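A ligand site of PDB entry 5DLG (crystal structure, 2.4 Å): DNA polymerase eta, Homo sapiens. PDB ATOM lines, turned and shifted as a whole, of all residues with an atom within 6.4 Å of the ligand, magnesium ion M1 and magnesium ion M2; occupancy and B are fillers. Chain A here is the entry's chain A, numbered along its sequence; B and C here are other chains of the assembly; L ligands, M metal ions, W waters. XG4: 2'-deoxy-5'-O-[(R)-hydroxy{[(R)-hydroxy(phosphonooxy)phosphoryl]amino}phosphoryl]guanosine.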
ATOM      1  N   VAL A  15      12.288   4.771 -18.507  1.00  0.00           N
ATOM      2  CA  VAL A  15      12.525   3.445 -17.990  1.00  0.00           C
ATOM      3  C   VAL A  15      12.639   2.424 -19.129  1.00  0.00           C
ATOM      4  O   VAL A  15      11.750   2.311 -19.965  1.00  0.00           O
ATOM      5  CB  VAL A  15      11.411   3.012 -17.042  1.00  0.00           C
ATOM      6  CG1 VAL A  15      11.668   1.598 -16.557  1.00  0.00           C
ATOM      7  CG2 VAL A  15      11.332   3.958 -15.857  1.00  0.00           C
ATOM      8  N   ASP A  16      13.725   1.676 -19.139  1.00  0.00           N
ATOM      9  CA  ASP A  16      13.927   0.685 -20.177  1.00  0.00           C
ATOM     10  C   ASP A  16      14.244  -0.690 -19.573  1.00  0.00           C
ATOM     11  O   ASP A  16      15.138  -0.812 -18.741  1.00  0.00           O
ATOM     12  CB  ASP A  16      15.053   1.142 -21.095  1.00  0.00           C
ATOM     13  CG  ASP A  16      15.195   0.266 -22.308  1.00  0.00           C
ATOM     14  OD1 ASP A  16      15.803  -0.819 -22.176  1.00  0.00           O
ATOM     15  OD2 ASP A  16      14.688   0.652 -23.388  1.00  0.00           O
ATOM     16  N   MET A  17      13.516  -1.720 -19.998  1.00  0.00           N
ATOM     17  CA  MET A  17      13.706  -3.091 -19.481  1.00  0.00           C
ATOM     18  C   MET A  17      15.052  -3.691 -19.902  1.00  0.00           C
ATOM     19  O   MET A  17      15.443  -3.584 -21.046  1.00  0.00           O
ATOM     20  CB  MET A  17      12.579  -4.015 -19.962  1.00  0.00           C
ATOM     21  CG  MET A  17      11.190  -3.444 -19.782  1.00  0.00           C
ATOM     22  SD  MET A  17      10.838  -2.978 -18.075  1.00  0.00           S
ATOM     23  CE  MET A  17      10.937  -4.546 -17.269  1.00  0.00           C
ATOM     24  N   ASP A  18      15.741  -4.303 -18.957  1.00  0.00           N
ATOM     25  CA  ASP A  18      17.007  -4.965 -19.270  1.00  0.00           C
ATOM     26  C   ASP A  18      16.765  -6.203 -20.131  1.00  0.00           C
ATOM     27  O   ASP A  18      15.911  -7.031 -19.793  1.00  0.00           O
ATOM     28  CB  ASP A  18      17.735  -5.344 -17.990  1.00  0.00           C
ATOM     29  CG  ASP A  18      18.094  -4.131 -17.144  1.00  0.00           C
ATOM     30  OD1 ASP A  18      18.239  -3.040 -17.710  1.00  0.00           O
ATOM     31  OD2 ASP A  18      18.252  -4.292 -15.912  1.00  0.00           O
ATOM     32  N   CYS A  19      17.520  -6.326 -21.228  1.00  0.00           N
ATOM     33  CA  CYS A  19      17.382  -7.427 -22.214  1.00  0.00           C
ATOM     34  C   CYS A  19      15.979  -8.068 -22.230  1.00  0.00           C
ATOM     35  O   CYS A  19      15.823  -9.243 -21.928  1.00  0.00           O
ATOM     36  CB  CYS A  19      18.457  -8.503 -21.957  1.00  0.00           C
ATOM     37  SG  CYS A  19      18.580  -9.171 -20.266  1.00  0.00           S
ATOM     38  N   PHE A  20      14.974  -7.259 -22.558  1.00  0.00           N
ATOM     39  CA  PHE A  20      13.579  -7.585 -22.291  1.00  0.00           C
ATOM     40  C   PHE A  20      13.081  -8.968 -22.798  1.00  0.00           C
ATOM     41  O   PHE A  20      12.554  -9.767 -22.012  1.00  0.00           O
ATOM     42  CB  PHE A  20      12.685  -6.475 -22.864  1.00  0.00           C
ATOM     43  CG  PHE A  20      11.246  -6.607 -22.466  1.00  0.00           C
ATOM     44  CD1 PHE A  20      10.897  -6.941 -21.157  1.00  0.00           C
ATOM     45  CD2 PHE A  20      10.228  -6.406 -23.391  1.00  0.00           C
ATOM     46  CE1 PHE A  20       9.589  -7.087 -20.774  1.00  0.00           C
ATOM     47  CE2 PHE A  20       8.888  -6.556 -23.005  1.00  0.00           C
ATOM     48  CZ  PHE A  20       8.581  -6.890 -21.701  1.00  0.00           C
ATOM     49  N   PHE A  21      13.251  -9.263 -24.082  1.00  0.00           N
ATOM     50  CA  PHE A  21      12.751 -10.555 -24.594  1.00  0.00           C
ATOM     51  C   PHE A  21      13.389 -11.737 -23.845  1.00  0.00           C
ATOM     52  O   PHE A  21      12.729 -12.726 -23.566  1.00  0.00           O
ATOM     53  CB  PHE A  21      12.967 -10.685 -26.108  1.00  0.00           C
ATOM     54  CG  PHE A  21      12.032  -9.835 -26.954  1.00  0.00           C
ATOM     55  CD1 PHE A  21      11.426  -8.698 -26.431  1.00  0.00           C
ATOM     56  CD2 PHE A  21      11.755 -10.182 -28.269  1.00  0.00           C
ATOM     57  CE1 PHE A  21      10.570  -7.896 -27.203  1.00  0.00           C
ATOM     58  CE2 PHE A  21      10.894  -9.393 -29.042  1.00  0.00           C
ATOM     59  CZ  PHE A  21      10.299  -8.231 -28.504  1.00  0.00           C
ATOM     60  N   VAL A  22      14.670 -11.623 -23.493  1.00  0.00           N
ATOM     61  CA  VAL A  22      15.378 -12.665 -22.737  1.00  0.00           C
ATOM     62  C   VAL A  22      14.785 -12.816 -21.327  1.00  0.00           C
ATOM     63  O   VAL A  22      14.476 -13.931 -20.890  1.00  0.00           O
ATOM     64  CB  VAL A  22      16.898 -12.391 -22.664  1.00  0.00           C
ATOM     65  CG1 VAL A  22      17.568 -13.201 -21.595  1.00  0.00           C
ATOM     66  CG2 VAL A  22      17.553 -12.709 -24.008  1.00  0.00           C
ATOM     67  N   GLN A  41      14.917 -15.543 -33.828  1.00  0.00           N
ATOM     68  CA  GLN A  41      13.774 -15.867 -34.674  1.00  0.00           C
ATOM     69  C   GLN A  41      14.260 -16.628 -35.917  1.00  0.00           C
ATOM     70  O   GLN A  41      15.268 -16.233 -36.536  1.00  0.00           O
ATOM     71  CB  GLN A  41      12.970 -14.599 -35.060  1.00  0.00           C
ATOM     72  CG  GLN A  41      13.802 -13.363 -35.325  1.00  0.00           C
ATOM     73  CD  GLN A  41      12.958 -12.104 -35.594  1.00  0.00           C
ATOM     74  OE1 GLN A  41      11.869 -11.933 -35.029  1.00  0.00           O
ATOM     75  NE2 GLN A  41      13.472 -11.220 -36.441  1.00  0.00           N
ATOM     76  N   ILE A  50      19.607 -13.230 -33.804  1.00  0.00           N
ATOM     77  CA  ILE A  50      19.486 -12.801 -32.418  1.00  0.00           C
ATOM     78  C   ILE A  50      18.891 -11.399 -32.312  1.00  0.00           C
ATOM     79  O   ILE A  50      19.340 -10.467 -32.983  1.00  0.00           O
ATOM     80  CB  ILE A  50      20.857 -12.839 -31.726  1.00  0.00           C
ATOM     81  CG1 ILE A  50      21.335 -14.278 -31.581  1.00  0.00           C
ATOM     82  CG2 ILE A  50      20.820 -12.153 -30.365  1.00  0.00           C
ATOM     83  CD1 ILE A  50      22.797 -14.350 -31.303  1.00  0.00           C
ATOM     84  N   ILE A  51      17.872 -11.257 -31.472  1.00  0.00           N
ATOM     85  CA  ILE A  51      17.238  -9.954 -31.257  1.00  0.00           C
ATOM     86  C   ILE A  51      17.325  -9.505 -29.798  1.00  0.00           C
ATOM     87  O   ILE A  51      17.083  -8.329 -29.508  1.00  0.00           O
ATOM     88  CB  ILE A  51      15.749  -9.959 -31.691  1.00  0.00           C
ATOM     89  CG1 ILE A  51      14.954 -11.009 -30.919  1.00  0.00           C
ATOM     90  CG2 ILE A  51      15.626 -10.212 -33.198  1.00  0.00           C
ATOM     91  CD1 ILE A  51      13.502 -11.066 -31.340  1.00  0.00           C
ATOM     92  N   ALA A  52      17.656 -10.404 -28.882  1.00  0.00           N
ATOM     93  CA  ALA A  52      17.902 -10.020 -27.502  1.00  0.00           C
ATOM     94  C   ALA A  52      19.022 -10.868 -26.868  1.00  0.00           C
ATOM     95  O   ALA A  52      19.091 -12.069 -27.107  1.00  0.00           O
ATOM     96  CB  ALA A  52      16.608 -10.127 -26.659  1.00  0.00           C
ATOM     97  N   VAL A  53      19.893 -10.228 -26.070  1.00  0.00           N
ATOM     98  CA  VAL A  53      21.052 -10.905 -25.494  1.00  0.00           C
ATOM     99  C   VAL A  53      21.159 -10.632 -23.997  1.00  0.00           C
ATOM    100  O   VAL A  53      21.138  -9.490 -23.570  1.00  0.00           O
ATOM    101  CB  VAL A  53      22.377 -10.439 -26.153  1.00  0.00           C
ATOM    102  CG1 VAL A  53      23.490 -11.356 -25.783  1.00  0.00           C
ATOM    103  CG2 VAL A  53      22.236 -10.349 -27.630  1.00  0.00           C
ATOM    104  N   TYR A  55      23.060 -10.149 -20.433  1.00  0.00           N
ATOM    105  CA  TYR A  55      24.339  -9.495 -20.189  1.00  0.00           C
ATOM    106  C   TYR A  55      25.488 -10.506 -19.947  1.00  0.00           C
ATOM    107  O   TYR A  55      26.626 -10.200 -20.253  1.00  0.00           O
ATOM    108  CB  TYR A  55      24.216  -8.509 -19.031  1.00  0.00           C
ATOM    109  CG  TYR A  55      23.471  -7.253 -19.432  1.00  0.00           C
ATOM    110  CD1 TYR A  55      22.090  -7.249 -19.569  1.00  0.00           C
ATOM    111  CD2 TYR A  55      24.149  -6.070 -19.672  1.00  0.00           C
ATOM    112  CE1 TYR A  55      21.406  -6.107 -19.931  1.00  0.00           C
ATOM    113  CE2 TYR A  55      23.480  -4.918 -20.034  1.00  0.00           C
ATOM    114  CZ  TYR A  55      22.113  -4.934 -20.175  1.00  0.00           C
ATOM    115  OH  TYR A  55      21.435  -3.771 -20.542  1.00  0.00           O
ATOM    116  N   ARG A  58      26.462 -11.172 -23.453  1.00  0.00           N
ATOM    117  CA  ARG A  58      27.101  -9.965 -23.965  1.00  0.00           C
ATOM    118  C   ARG A  58      28.595  -9.911 -23.612  1.00  0.00           C
ATOM    119  O   ARG A  58      29.382  -9.333 -24.354  1.00  0.00           O
ATOM    120  CB  ARG A  58      26.410  -8.709 -23.421  1.00  0.00           C
ATOM    121  CG  ARG A  58      24.974  -8.522 -23.869  1.00  0.00           C
ATOM    122  CD  ARG A  58      24.382  -7.177 -23.369  1.00  0.00           C
ATOM    123  NE  ARG A  58      22.938  -7.108 -23.586  1.00  0.00           N
ATOM    124  CZ  ARG A  58      22.210  -5.999 -23.568  1.00  0.00           C
ATOM    125  NH1 ARG A  58      22.770  -4.813 -23.359  1.00  0.00           N
ATOM    126  NH2 ARG A  58      20.892  -6.065 -23.768  1.00  0.00           N
ATOM    127  N   ARG A  64      22.949  -8.272 -30.610  1.00  0.00           N
ATOM    128  CA  ARG A  64      21.830  -8.157 -31.520  1.00  0.00           C
ATOM    129  C   ARG A  64      22.320  -8.260 -32.967  1.00  0.00           C
ATOM    130  O   ARG A  64      23.451  -7.847 -33.276  1.00  0.00           O
ATOM    131  CB  ARG A  64      21.112  -6.826 -31.280  1.00  0.00           C
ATOM    132  CG  ARG A  64      19.968  -6.588 -32.210  1.00  0.00           C
ATOM    133  CD  ARG A  64      19.146  -5.365 -31.842  1.00  0.00           C
ATOM    134  NE  ARG A  64      18.126  -5.185 -32.884  1.00  0.00           N
ATOM    135  CZ  ARG A  64      18.295  -4.413 -33.957  1.00  0.00           C
ATOM    136  NH1 ARG A  64      19.428  -3.719 -34.101  1.00  0.00           N
ATOM    137  NH2 ARG A  64      17.327  -4.320 -34.870  1.00  0.00           N
ATOM    138  N   ALA A  90       7.079 -14.808 -37.559  1.00  0.00           N
ATOM    139  CA  ALA A  90       7.349 -14.379 -36.199  1.00  0.00           C
ATOM    140  C   ALA A  90       6.079 -13.857 -35.571  1.00  0.00           C
ATOM    141  O   ALA A  90       5.311 -13.132 -36.211  1.00  0.00           O
ATOM    142  CB  ALA A  90       8.417 -13.312 -36.183  1.00  0.00           C
ATOM    143  N   LEU A  92       4.920 -11.957 -32.048  1.00  0.00           N
ATOM    144  CA  LEU A  92       5.519 -11.321 -30.893  1.00  0.00           C
ATOM    145  C   LEU A  92       4.542 -11.155 -29.739  1.00  0.00           C
ATOM    146  O   LEU A  92       4.783 -10.378 -28.819  1.00  0.00           O
ATOM    147  CB  LEU A  92       6.122  -9.960 -31.271  1.00  0.00           C
ATOM    148  CG  LEU A  92       7.203 -10.009 -32.358  1.00  0.00           C
ATOM    149  CD1 LEU A  92       7.747  -8.621 -32.613  1.00  0.00           C
ATOM    150  CD2 LEU A  92       8.314 -10.943 -31.961  1.00  0.00           C
ATOM    151  N   SER A 116       8.475   2.312 -26.896  1.00  0.00           N
ATOM    152  CA  SER A 116       8.800   1.092 -27.628  1.00  0.00           C
ATOM    153  C   SER A 116       8.070  -0.030 -26.905  1.00  0.00           C
ATOM    154  O   SER A 116       7.403   0.242 -25.922  1.00  0.00           O
ATOM    155  CB  SER A 116      10.316   0.835 -27.667  1.00  0.00           C
ATOM    156  OG  SER A 116      10.810   0.485 -26.381  1.00  0.00           O
ATOM    157  N   ILE A 117       8.216  -1.258 -27.368  1.00  0.00           N
ATOM    158  CA  ILE A 117       7.633  -2.387 -26.647  1.00  0.00           C
ATOM    159  C   ILE A 117       8.190  -2.492 -25.207  1.00  0.00           C
ATOM    160  O   ILE A 117       7.531  -3.056 -24.340  1.00  0.00           O
ATOM    161  CB  ILE A 117       7.891  -3.712 -27.375  1.00  0.00           C
ATOM    162  CG1 ILE A 117       6.977  -4.832 -26.833  1.00  0.00           C
ATOM    163  CG2 ILE A 117       9.383  -4.101 -27.339  1.00  0.00           C
ATOM    164  CD1 ILE A 117       6.774  -5.953 -27.857  1.00  0.00           C
ATOM    165  N   ASP A 118       9.346  -1.884 -24.969  1.00  0.00           N
ATOM    166  CA  ASP A 118      10.180  -2.136 -23.780  1.00  0.00           C
ATOM    167  C   ASP A 118      10.340  -0.902 -22.883  1.00  0.00           C
ATOM    168  O   ASP A 118      10.627  -1.038 -21.697  1.00  0.00           O
ATOM    169  CB  ASP A 118      11.530  -2.686 -24.297  1.00  0.00           C
ATOM    170  CG  ASP A 118      12.741  -2.435 -23.394  1.00  0.00           C
ATOM    171  OD1 ASP A 118      12.831  -1.501 -22.578  1.00  0.00           O
ATOM    172  OD2 ASP A 118      13.680  -3.238 -23.488  1.00  0.00           O
ATOM    173  N   GLU A 119      10.178   0.310 -23.419  1.00  0.00           N
ATOM    174  CA  GLU A 119      10.428   1.504 -22.621  1.00  0.00           C
ATOM    175  C   GLU A 119       9.306   2.525 -22.694  1.00  0.00           C
ATOM    176  O   GLU A 119       8.530   2.538 -23.649  1.00  0.00           O
ATOM    177  CB  GLU A 119      11.739   2.178 -23.050  1.00  0.00           C
ATOM    178  CG  GLU A 119      11.703   2.788 -24.434  1.00  0.00           C
ATOM    179  CD  GLU A 119      12.992   2.539 -25.206  1.00  0.00           C
ATOM    180  OE1 GLU A 119      13.732   3.507 -25.474  1.00  0.00           O
ATOM    181  OE2 GLU A 119      13.264   1.379 -25.547  1.00  0.00           O
ATOM    182  N   SER A 216      16.287  -0.628 -16.189  1.00  0.00           N
ATOM    183  CA  SER A 216      17.085   0.549 -15.856  1.00  0.00           C
ATOM    184  C   SER A 216      16.310   1.830 -16.144  1.00  0.00           C
ATOM    185  O   SER A 216      15.320   1.804 -16.845  1.00  0.00           O
ATOM    186  CB  SER A 216      18.399   0.523 -16.614  1.00  0.00           C
ATOM    187  OG  SER A 216      19.103  -0.648 -16.265  1.00  0.00           O
ATOM    188  N   LYS A 227      16.902   9.481 -21.557  1.00  0.00           N
ATOM    189  CA  LYS A 227      17.213   8.326 -22.402  1.00  0.00           C
ATOM    190  C   LYS A 227      18.703   8.007 -22.394  1.00  0.00           C
ATOM    191  O   LYS A 227      19.079   6.871 -22.193  1.00  0.00           O
ATOM    192  CB  LYS A 227      16.725   8.564 -23.828  1.00  0.00           C
ATOM    193  CG  LYS A 227      17.157   7.490 -24.841  1.00  0.00           C
ATOM    194  CD  LYS A 227      16.510   6.137 -24.572  1.00  0.00           C
ATOM    195  CE  LYS A 227      16.927   5.094 -25.615  1.00  0.00           C
ATOM    196  NZ  LYS A 227      16.317   3.758 -25.348  1.00  0.00           N
ATOM    197  N   LYS A 234      23.336   0.635 -17.165  1.00  0.00           N
ATOM    198  CA  LYS A 234      22.701  -0.654 -17.355  1.00  0.00           C
ATOM    199  C   LYS A 234      23.699  -1.748 -16.999  1.00  0.00           C
ATOM    200  O   LYS A 234      24.897  -1.560 -17.195  1.00  0.00           O
ATOM    201  CB  LYS A 234      22.215  -0.806 -18.807  1.00  0.00           C
ATOM    202  CG  LYS A 234      20.897  -0.124 -19.081  1.00  0.00           C
ATOM    203  CD  LYS A 234      20.275  -0.458 -20.452  1.00  0.00           C
ATOM    204  CE  LYS A 234      18.775  -0.097 -20.476  1.00  0.00           C
ATOM    205  NZ  LYS A 234      17.881  -1.296 -20.215  1.00  0.00           N
ATOM    206  N   PRO A 235      23.225  -2.887 -16.461  1.00  0.00           N
ATOM    207  CA  PRO A 235      21.838  -3.242 -16.134  1.00  0.00           C
ATOM    208  C   PRO A 235      21.423  -3.015 -14.682  1.00  0.00           C
ATOM    209  O   PRO A 235      22.267  -2.800 -13.803  1.00  0.00           O
ATOM    210  CB  PRO A 235      21.832  -4.745 -16.411  1.00  0.00           C
ATOM    211  CG  PRO A 235      23.210  -5.156 -15.908  1.00  0.00           C
ATOM    212  CD  PRO A 235      24.107  -4.069 -16.416  1.00  0.00           C
ATOM    213  P    DT B   8      17.549   3.047 -30.200  1.00  0.00           P
ATOM    214  OP1  DT B   8      17.857   3.522 -28.825  1.00  0.00           O
ATOM    215  OP2  DT B   8      18.623   2.530 -31.099  1.00  0.00           O
ATOM    216  O5'  DT B   8      16.405   1.947 -29.982  1.00  0.00           O
ATOM    217  C5'  DT B   8      15.144   2.356 -29.404  1.00  0.00           C
ATOM    218  C4'  DT B   8      14.201   1.179 -29.315  1.00  0.00           C
ATOM    219  O4'  DT B   8      13.881   0.721 -30.659  1.00  0.00           O
ATOM    220  C3'  DT B   8      14.805  -0.027 -28.601  1.00  0.00           C
ATOM    221  O3'  DT B   8      13.842  -0.631 -27.672  1.00  0.00           O
ATOM    222  C2'  DT B   8      15.220  -0.972 -29.749  1.00  0.00           C
ATOM    223  C1'  DT B   8      14.183  -0.651 -30.803  1.00  0.00           C
ATOM    224  N1   DT B   8      14.635  -0.879 -32.216  1.00  0.00           N
ATOM    225  C2   DT B   8      13.823  -1.602 -33.080  1.00  0.00           C
ATOM    226  O2   DT B   8      12.764  -2.095 -32.737  1.00  0.00           O
ATOM    227  N3   DT B   8      14.316  -1.733 -34.358  1.00  0.00           N
ATOM    228  C4   DT B   8      15.504  -1.237 -34.850  1.00  0.00           C
ATOM    229  O4   DT B   8      15.852  -1.400 -36.018  1.00  0.00           O
ATOM    230  C5   DT B   8      16.297  -0.483 -33.896  1.00  0.00           C
ATOM    231  C7   DT B   8      17.607   0.123 -34.310  1.00  0.00           C
ATOM    232  C6   DT B   8      15.825  -0.343 -32.633  1.00  0.00           C
ATOM    233  P    DA C   5      10.707 -10.755 -40.661  1.00  0.00           P
ATOM    234  OP1  DA C   5      10.106 -12.099 -40.768  1.00  0.00           O
ATOM    235  OP2  DA C   5      10.709  -9.865 -41.841  1.00  0.00           O
ATOM    236  O5'  DA C   5       9.993  -9.968 -39.507  1.00  0.00           O
ATOM    237  C5'  DA C   5       9.882 -10.564 -38.221  1.00  0.00           C
ATOM    238  C4'  DA C   5       9.281  -9.603 -37.224  1.00  0.00           C
ATOM    239  O4'  DA C   5      10.213  -8.515 -36.942  1.00  0.00           O
ATOM    240  C3'  DA C   5       7.982  -8.933 -37.643  1.00  0.00           C
ATOM    241  O3'  DA C   5       7.156  -8.870 -36.523  1.00  0.00           O
ATOM    242  C2'  DA C   5       8.445  -7.539 -38.111  1.00  0.00           C
ATOM    243  C1'  DA C   5       9.598  -7.264 -37.150  1.00  0.00           C
ATOM    244  N9   DA C   5      10.604  -6.380 -37.675  1.00  0.00           N
ATOM    245  C8   DA C   5      11.133  -6.382 -38.937  1.00  0.00           C
ATOM    246  N7   DA C   5      12.060  -5.492 -39.126  1.00  0.00           N
ATOM    247  C5   DA C   5      12.180  -4.852 -37.900  1.00  0.00           C
ATOM    248  C6   DA C   5      12.990  -3.785 -37.444  1.00  0.00           C
ATOM    249  N6   DA C   5      13.892  -3.169 -38.222  1.00  0.00           N
ATOM    250  N1   DA C   5      12.842  -3.391 -36.166  1.00  0.00           N
ATOM    251  C2   DA C   5      11.947  -4.016 -35.396  1.00  0.00           C
ATOM    252  N3   DA C   5      11.115  -5.018 -35.707  1.00  0.00           N
ATOM    253  C4   DA C   5      11.292  -5.391 -36.986  1.00  0.00           C
HETATM  254  N1  XG4 L   1      13.693  -7.181 -34.380  1.00  0.00           N
HETATM  255  C2  XG4 L   1      12.800  -7.614 -33.455  1.00  0.00           C
HETATM  256  N2  XG4 L   1      11.823  -8.495 -33.803  1.00  0.00           N
HETATM  257  N3  XG4 L   1      12.854  -7.195 -32.159  1.00  0.00           N
HETATM  258  C4  XG4 L   1      13.814  -6.329 -31.739  1.00  0.00           C
HETATM  259  C5  XG4 L   1      14.807  -5.816 -32.688  1.00  0.00           C
HETATM  260  C6  XG4 L   1      14.677  -6.321 -34.085  1.00  0.00           C
HETATM  261  O6  XG4 L   1      15.479  -5.949 -34.979  1.00  0.00           O
HETATM  262  N7  XG4 L   1      15.613  -4.982 -31.991  1.00  0.00           N
HETATM  263  C8  XG4 L   1      15.171  -4.952 -30.706  1.00  0.00           C
HETATM  264  N9  XG4 L   1      14.093  -5.771 -30.552  1.00  0.00           N
HETATM  265  PA  XG4 L   1      16.145  -2.772 -26.464  1.00  0.00           P
HETATM  266  PB  XG4 L   1      17.075  -4.994 -24.739  1.00  0.00           P
HETATM  267  PG  XG4 L   1      18.828  -3.442 -23.121  1.00  0.00           P
HETATM  268  C1' XG4 L   1      13.295  -6.069 -29.344  1.00  0.00           C
HETATM  269  O1A XG4 L   1      15.811  -2.111 -25.190  1.00  0.00           O
HETATM  270  O1B XG4 L   1      15.924  -4.493 -23.969  1.00  0.00           O
HETATM  271  O1G XG4 L   1      17.694  -2.466 -23.247  1.00  0.00           O
HETATM  272  C2' XG4 L   1      14.058  -7.085 -28.484  1.00  0.00           C
HETATM  273  O2A XG4 L   1      16.937  -1.796 -27.459  1.00  0.00           O
HETATM  274  O2B XG4 L   1      16.855  -6.530 -25.090  1.00  0.00           O
HETATM  275  O2G XG4 L   1      20.132  -2.934 -23.724  1.00  0.00           O
HETATM  276  C3' XG4 L   1      14.463  -6.257 -27.282  1.00  0.00           C
HETATM  277  O3' XG4 L   1      14.537  -7.025 -26.083  1.00  0.00           O
HETATM  278  N3A XG4 L   1      17.252  -4.112 -26.252  1.00  0.00           N
HETATM  279  O3B XG4 L   1      18.438  -4.808 -23.887  1.00  0.00           O
HETATM  280  O3G XG4 L   1      19.049  -3.752 -21.675  1.00  0.00           O
HETATM  281  C4' XG4 L   1      13.358  -5.224 -27.183  1.00  0.00           C
HETATM  282  O4' XG4 L   1      13.044  -4.910 -28.541  1.00  0.00           O
HETATM  283  C5' XG4 L   1      13.818  -3.987 -26.438  1.00  0.00           C
HETATM  284  O5' XG4 L   1      14.822  -3.305 -27.177  1.00  0.00           O
HETATM  285 MG    MG M   1      15.565  -2.574 -22.962  1.00  0.00          MG
HETATM  286 MG    MG M   2      13.947  -0.385 -25.199  1.00  0.00          MG
HETATM  287  O   HOH W   1      15.768   0.465 -25.762  1.00  0.00           O
HETATM  288  O   HOH W   2      20.652  -3.271 -26.313  1.00  0.00           O
HETATM  289  O   HOH W   3      13.739  -8.147 -37.079  1.00  0.00           O
HETATM  290  O   HOH W   4      22.929  -1.123 -22.901  1.00  0.00           O
HETATM  291  O   HOH W   5      15.421  -6.351 -37.815  1.00  0.00           O
HETATM  292  O   HOH W   6      18.374  -5.442 -28.591  1.00  0.00           O
HETATM  293  O   HOH W   7      18.098  -0.137 -24.369  1.00  0.00           O
HETATM  294  O   HOH W   8      19.296  -7.438 -25.620  1.00  0.00           O
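Merely in contact with magnesium ion M2: Ser 116.
Within 4 Å of magnesium ion M2: Asp 16, Ser 116, Asp 118, Glu 119 and DT 8 of chain B.
Magnesium ion M2 is bound by OE2 of Glu 119 (1.9 Å), water W1 (2.1 Å), OD2 of Asp 16 (2.2 Å), O3' of DT 8 of chain B (2.5 Å) and O1A of the ligand (2.5 Å).
Water W1 lies within hydrogen-bond range of O2A of the ligand (3.1 Å) and NZ of Lys 227 (3.4 Å).
Water W8 lies within hydrogen-bond range of O2B of the ligand (2.7 Å), NH2 of Arg 58 (2.8 Å) and N of Val 53 (2.9 Å).
Water W3 lies within hydrogen-bond range of N1 of the ligand and NE2 of Gln 41.
Water W6 lies within hydrogen-bond range of a nitrogen (N3A) of the ligand (2.9 Å) and the backbone carbonyl oxygen of Ile 51 (3.3 Å).
NZ of Lys 234 touches magnesium ion M1 (3.8 Å).
Within 4 Å of magnesium ion M1: Asp 16, Met 17, Asp 118 and Lys 234.
Magnesium ion M1 is bound by the side-chain carboxylate (OD1) of Asp 16 (1.9 Å), the side-chain carboxylate (OD2) of Asp 118 (2.1 Å), an oxygen (O1G) of the ligand (2.2 Å), the backbone carbonyl oxygen (O) of Met 17 (2.2 Å), an oxygen (O1B) of the ligand (2.2 Å) and an oxygen (O1A) of the ligand (2.3 Å).
Magnesium ion M1 has six donor atoms within binding distance.
The backbone NH (N) of Phe 21 is in hydrogen-bond range of an oxygen (O3') of the ligand (3.3 Å).
O3G of the ligand is in salt-bridge range of NZ of Lys 234.
NH2 of Arg 64 is in hydrogen-bond range of O6 of the ligand (2.5 Å).
The backbone NH (N) of Cys 19 is in hydrogen-bond range of an oxygen (O3G) of the ligand.
An oxygen (O3G) of the ligand lies within hydrogen-bond range of the side-chain hydroxyl (OH) of Tyr 55 (2.6 Å).
The backbone NH of Phe 20 sits at hydrogen-bond distance from an oxygen (O2B) of the ligand (3.2 Å).
The guanidinium group (NH2) of Arg 58 is in salt-bridge range of an oxygen (O2G) of the ligand (3.2 Å).
The side-chain carboxylate (OE1) of Glu 119 lies within salt-bridge range of the side-chain amino group (NZ) of Lys 227 (2.6 Å).
The side-chain amino group (NZ) of Lys 234 lies within salt-bridge range of the side-chain carboxylate (OD1) of Asp 18 (3.1 Å).
The side-chain hydroxyl of Ser 216 sits at hydrogen-bond distance from the side-chain carboxylate of Asp 18 (2.9 Å).
N of Asp 16 is in hydrogen-bond range of O of Ser 216 (2.8 Å).
O3' of DT 8 of chain B sits close to OG of Ser 116, 3.5 Å away.
The side-chain amino group (NZ) of Lys 234 is in hydrogen-bond range of the backbone carbonyl oxygen (O) of Asp 16.
O4 of DT 8 of chain B lies within hydrogen-bond range of the guanidinium group of Arg 64.
NE of Arg 58 sits at hydrogen-bond distance from O of Val 53 (3.0 Å).
Asp 18 touches the ligand.
Gln 41 touches the ligand.
Ile 51 touches the ligand.
Ala 52 touches the ligand (CB to O3', 3.8 Å).
CG2 of Ile 117 touches O4' of the ligand, 3.9 Å away.
DA 5 of chain C touches the ligand (O4' to N2, 3.5 Å).
Hydrophobic or aromatic side chains within 4 Å of the ligand: Phe 20, Phe 21, Ile 51, Ala 52, Tyr 55 and Ile 117.
Within 4 Å of the ligand: Asp 16, Met 17, Asp 18, Cys 19, Phe 20, Phe 21, Gln 41, Ile 51, Ala 52, Tyr 55, Arg 58, Arg 64, Ile 117, Asp 118, Lys 234, DT 8 of chain B and DA 5 of chain C.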
